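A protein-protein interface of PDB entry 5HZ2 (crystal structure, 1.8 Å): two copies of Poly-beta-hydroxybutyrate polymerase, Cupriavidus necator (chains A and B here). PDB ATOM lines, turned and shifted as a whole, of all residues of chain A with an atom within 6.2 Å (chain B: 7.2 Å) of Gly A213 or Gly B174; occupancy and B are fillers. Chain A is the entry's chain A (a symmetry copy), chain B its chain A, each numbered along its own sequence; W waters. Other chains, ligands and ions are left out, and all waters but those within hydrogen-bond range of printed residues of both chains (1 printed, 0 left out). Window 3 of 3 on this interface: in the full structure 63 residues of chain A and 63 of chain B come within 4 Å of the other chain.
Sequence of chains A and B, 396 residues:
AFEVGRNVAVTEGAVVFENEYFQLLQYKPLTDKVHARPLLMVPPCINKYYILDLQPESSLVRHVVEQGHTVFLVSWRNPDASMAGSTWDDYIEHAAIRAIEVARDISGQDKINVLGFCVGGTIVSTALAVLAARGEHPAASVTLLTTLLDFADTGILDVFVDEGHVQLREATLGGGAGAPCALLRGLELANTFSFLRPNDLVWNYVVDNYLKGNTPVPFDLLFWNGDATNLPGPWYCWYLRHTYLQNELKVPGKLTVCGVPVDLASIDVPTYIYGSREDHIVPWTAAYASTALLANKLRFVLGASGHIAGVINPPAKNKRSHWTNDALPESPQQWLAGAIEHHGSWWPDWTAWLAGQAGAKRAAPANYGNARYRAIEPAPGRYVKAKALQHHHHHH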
ATOM      1  N   ASP A 208      -0.014  27.516  13.100  1.00  0.00           N
ATOM      2  CA  ASP A 208      -1.467  27.338  13.163  1.00  0.00           C
ATOM      3  C   ASP A 208      -1.887  26.296  12.072  1.00  0.00           C
ATOM      4  O   ASP A 208      -2.629  25.332  12.337  1.00  0.00           O
ATOM      5  CB  ASP A 208      -2.162  28.652  12.907  1.00  0.00           C
ATOM      6  CG  ASP A 208      -3.667  28.551  13.090  1.00  0.00           C
ATOM      7  OD1 ASP A 208      -4.128  28.246  14.202  1.00  0.00           O
ATOM      8  OD2 ASP A 208      -4.351  28.752  12.083  1.00  0.00           O
ATOM      9  N   ASN A 209      -1.361  26.477  10.886  1.00  0.00           N
ATOM     10  CA  ASN A 209      -1.681  25.561   9.796  1.00  0.00           C
ATOM     11  C   ASN A 209      -1.194  24.110  10.076  1.00  0.00           C
ATOM     12  O   ASN A 209      -1.900  23.110   9.825  1.00  0.00           O
ATOM     13  CB  ASN A 209      -1.033  26.136   8.591  1.00  0.00           C
ATOM     14  CG  ASN A 209      -1.606  25.616   7.347  1.00  0.00           C
ATOM     15  OD1 ASN A 209      -2.663  26.058   6.920  1.00  0.00           O
ATOM     16  ND2 ASN A 209      -0.923  24.662   6.756  1.00  0.00           N
ATOM     17  N   TYR A 210       0.011  23.985  10.599  1.00  0.00           N
ATOM     18  CA  TYR A 210       0.519  22.664  10.900  1.00  0.00           C
ATOM     19  C   TYR A 210      -0.307  21.971  11.983  1.00  0.00           C
ATOM     20  O   TYR A 210      -0.634  20.817  11.864  1.00  0.00           O
ATOM     21  CB  TYR A 210       1.991  22.715  11.305  1.00  0.00           C
ATOM     22  CG  TYR A 210       2.492  21.435  11.915  1.00  0.00           C
ATOM     23  CD1 TYR A 210       2.959  20.411  11.129  1.00  0.00           C
ATOM     24  CD2 TYR A 210       2.473  21.252  13.273  1.00  0.00           C
ATOM     25  CE1 TYR A 210       3.408  19.241  11.687  1.00  0.00           C
ATOM     26  CE2 TYR A 210       2.917  20.083  13.838  1.00  0.00           C
ATOM     27  CZ  TYR A 210       3.377  19.081  13.034  1.00  0.00           C
ATOM     28  OH  TYR A 210       3.819  17.923  13.600  1.00  0.00           O
ATOM     29  N   LEU A 211      -0.650  22.696  13.036  1.00  0.00           N
ATOM     30  CA  LEU A 211      -1.417  22.083  14.115  1.00  0.00           C
ATOM     31  C   LEU A 211      -2.771  21.594  13.649  1.00  0.00           C
ATOM     32  O   LEU A 211      -3.188  20.511  13.980  1.00  0.00           O
ATOM     33  CB  LEU A 211      -1.593  23.050  15.278  1.00  0.00           C
ATOM     34  CG  LEU A 211      -0.339  23.375  16.080  1.00  0.00           C
ATOM     35  CD1 LEU A 211      -0.558  24.465  17.100  1.00  0.00           C
ATOM     36  CD2 LEU A 211       0.343  22.159  16.672  1.00  0.00           C
ATOM     37  N   LYS A 212      -3.437  22.408  12.854  1.00  0.00           N
ATOM     38  CA  LYS A 212      -4.750  22.059  12.350  1.00  0.00           C
ATOM     39  C   LYS A 212      -4.759  20.839  11.468  1.00  0.00           C
ATOM     40  O   LYS A 212      -5.678  20.064  11.517  1.00  0.00           O
ATOM     41  CB  LYS A 212      -5.365  23.231  11.613  1.00  0.00           C
ATOM     42  CG  LYS A 212      -5.733  24.365  12.534  1.00  0.00           C
ATOM     43  CD  LYS A 212      -6.612  25.367  11.827  1.00  0.00           C
ATOM     44  CE  LYS A 212      -6.371  26.768  12.320  1.00  0.00           C
ATOM     45  NZ  LYS A 212      -7.352  27.168  13.357  1.00  0.00           N
ATOM     46  N   GLY A 213      -3.744  20.701  10.637  1.00  0.00           N
ATOM     47  CA  GLY A 213      -3.674  19.577   9.740  1.00  0.00           C
ATOM     48  C   GLY A 213      -2.960  18.329  10.191  1.00  0.00           C
ATOM     49  O   GLY A 213      -3.174  17.274   9.640  1.00  0.00           O
ATOM     50  N   ASN A 214      -2.096  18.450  11.176  1.00  0.00           N
ATOM     51  CA  ASN A 214      -1.333  17.308  11.621  1.00  0.00           C
ATOM     52  C   ASN A 214      -1.406  16.878  13.070  1.00  0.00           C
ATOM     53  O   ASN A 214      -0.696  16.007  13.465  1.00  0.00           O
ATOM     54  CB  ASN A 214       0.112  17.519  11.215  1.00  0.00           C
ATOM     55  CG  ASN A 214       0.244  17.856   9.749  1.00  0.00           C
ATOM     56  OD1 ASN A 214       0.370  16.972   8.927  1.00  0.00           O
ATOM     57  ND2 ASN A 214       0.193  19.125   9.423  1.00  0.00           N
ATOM     58  N   THR A 215      -2.262  17.509  13.851  1.00  0.00           N
ATOM     59  CA  THR A 215      -2.377  17.182  15.247  1.00  0.00           C
ATOM     60  C   THR A 215      -3.806  17.267  15.722  1.00  0.00           C
ATOM     61  O   THR A 215      -4.642  17.881  15.095  1.00  0.00           O
ATOM     62  CB  THR A 215      -1.568  18.145  16.153  1.00  0.00           C
ATOM     63  OG1 THR A 215      -2.249  19.395  16.285  1.00  0.00           O
ATOM     64  CG2 THR A 215      -0.190  18.373  15.635  1.00  0.00           C
ATOM     65  N   THR B 172     -10.104  11.023  13.422  1.00  0.00           N
ATOM     66  CA  THR B 172      -9.054  11.174  12.441  1.00  0.00           C
ATOM     67  C   THR B 172      -8.511  12.573  12.513  1.00  0.00           C
ATOM     68  O   THR B 172      -9.176  13.483  12.971  1.00  0.00           O
ATOM     69  CB  THR B 172      -9.569  10.922  11.009  1.00  0.00           C
ATOM     70  OG1 THR B 172      -8.497  11.080  10.077  1.00  0.00           O
ATOM     71  CG2 THR B 172     -10.648  11.907  10.660  1.00  0.00           C
ATOM     72  N   LEU B 173      -7.283  12.736  12.057  1.00  0.00           N
ATOM     73  CA  LEU B 173      -6.650  14.094  12.053  1.00  0.00           C
ATOM     74  C   LEU B 173      -7.275  14.967  10.939  1.00  0.00           C
ATOM     75  O   LEU B 173      -8.031  14.460  10.120  1.00  0.00           O
ATOM     76  CB  LEU B 173      -5.117  14.015  11.869  1.00  0.00           C
ATOM     77  CG  LEU B 173      -4.263  13.392  12.976  1.00  0.00           C
ATOM     78  CD1 LEU B 173      -2.779  13.416  12.566  1.00  0.00           C
ATOM     79  CD2 LEU B 173      -4.516  14.093  14.303  1.00  0.00           C
ATOM     80  N   GLY B 174      -6.970  16.269  10.923  1.00  0.00           N
ATOM     81  CA  GLY B 174      -7.382  17.189   9.825  1.00  0.00           C
ATOM     82  C   GLY B 174      -6.770  16.867   8.450  1.00  0.00           C
ATOM     83  O   GLY B 174      -7.460  16.943   7.433  1.00  0.00           O
ATOM     84  N   GLY B 175      -5.484  16.543   8.446  1.00  0.00           N
ATOM     85  CA  GLY B 175      -4.741  16.080   7.290  1.00  0.00           C
ATOM     86  C   GLY B 175      -4.504  16.960   6.090  1.00  0.00           C
ATOM     87  O   GLY B 175      -4.064  16.478   5.055  1.00  0.00           O
ATOM     88  N   GLY B 176      -4.832  18.234   6.188  1.00  0.00           N
ATOM     89  CA  GLY B 176      -4.672  19.116   5.053  1.00  0.00           C
ATOM     90  C   GLY B 176      -3.285  19.544   4.618  1.00  0.00           C
ATOM     91  O   GLY B 176      -2.337  19.580   5.408  1.00  0.00           O
ATOM     92  N   ALA B 177      -3.173  19.859   3.331  1.00  0.00           N
ATOM     93  CA  ALA B 177      -1.941  20.375   2.771  1.00  0.00           C
ATOM     94  C   ALA B 177      -1.932  21.801   3.311  1.00  0.00           C
ATOM     95  O   ALA B 177      -2.973  22.443   3.388  1.00  0.00           O
ATOM     96  CB  ALA B 177      -1.989  20.368   1.257  1.00  0.00           C
HETATM   97  O   HOH W   1      -5.876  17.807  12.636  1.00  0.00           O
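Among the printed residues, merely in contact across the chains: Asn A214 with Leu B173 (3.4 Å), Thr A215 with Leu B173 (3.5 Å), Lys A212 with Gly B174 (3.7 Å), Gly A213 with Gly B174 (3.8 Å) and Gly A213 with Gly B176 (3.9 Å).
Water W1 lies within hydrogen-bond range of the backbone carbonyl oxygen (O) of Lys A212 (2.5 Å), the backbone NH (N) of Gly B174 (2.5 Å) and the backbone carbonyl oxygen (O) of Thr A215 (2.8 Å).
Leu A211 touches none of the printed residues of chain B.
Printed residues of chain B within 4 Å of Lys A212: Gly B174 (3.7 Å).
Of chain B, only Gly B174, Gly B175 and Gly B176 come within 4 Å of Gly A213.
Printed residues of chain A within 4 Å of Leu B173: Asn A214 and Thr A215.
Gly B174 touches two residues of chain A.
Of the printed residues of chain A, Gly B176 touches Gly A213 (3.9 Å).
No position is printed for both chains.
Of the 6 pairs that touch across the chains among the printed residues, none has its exchanged pair printed and touching as well.
Printed residues of chain A that touch a printed residue of chain B: Lys A212, Gly A213, Asn A214 and Thr A215.
Along chain A the printed residues that touch a printed residue of chain B span positions 212 to 215.
Of the 6 printed residues of chain B, 4 touch a printed residue of chain A.
Among the printed residues, 6 pairs touch across the chains.
Among the printed residues, no Asp or Glu carboxylate lies within 4 Å of a Lys or Arg side-chain nitrogen of the other chain.
The side-chain carboxylate of Asp A208 lies within salt-bridge range of the side-chain amino group of Lys A212 (3.5 Å).
The backbone carbonyl oxygen of Tyr A210 is in hydrogen-bond range of the side-chain amide nitrogen of Asn A214 (3.1 Å).
O of Leu A211 is in hydrogen-bond range of OG1 of Thr A215 (2.7 Å).
N of Gly B175 sits at hydrogen-bond distance from O of Gly A213, at 2.7 Å.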
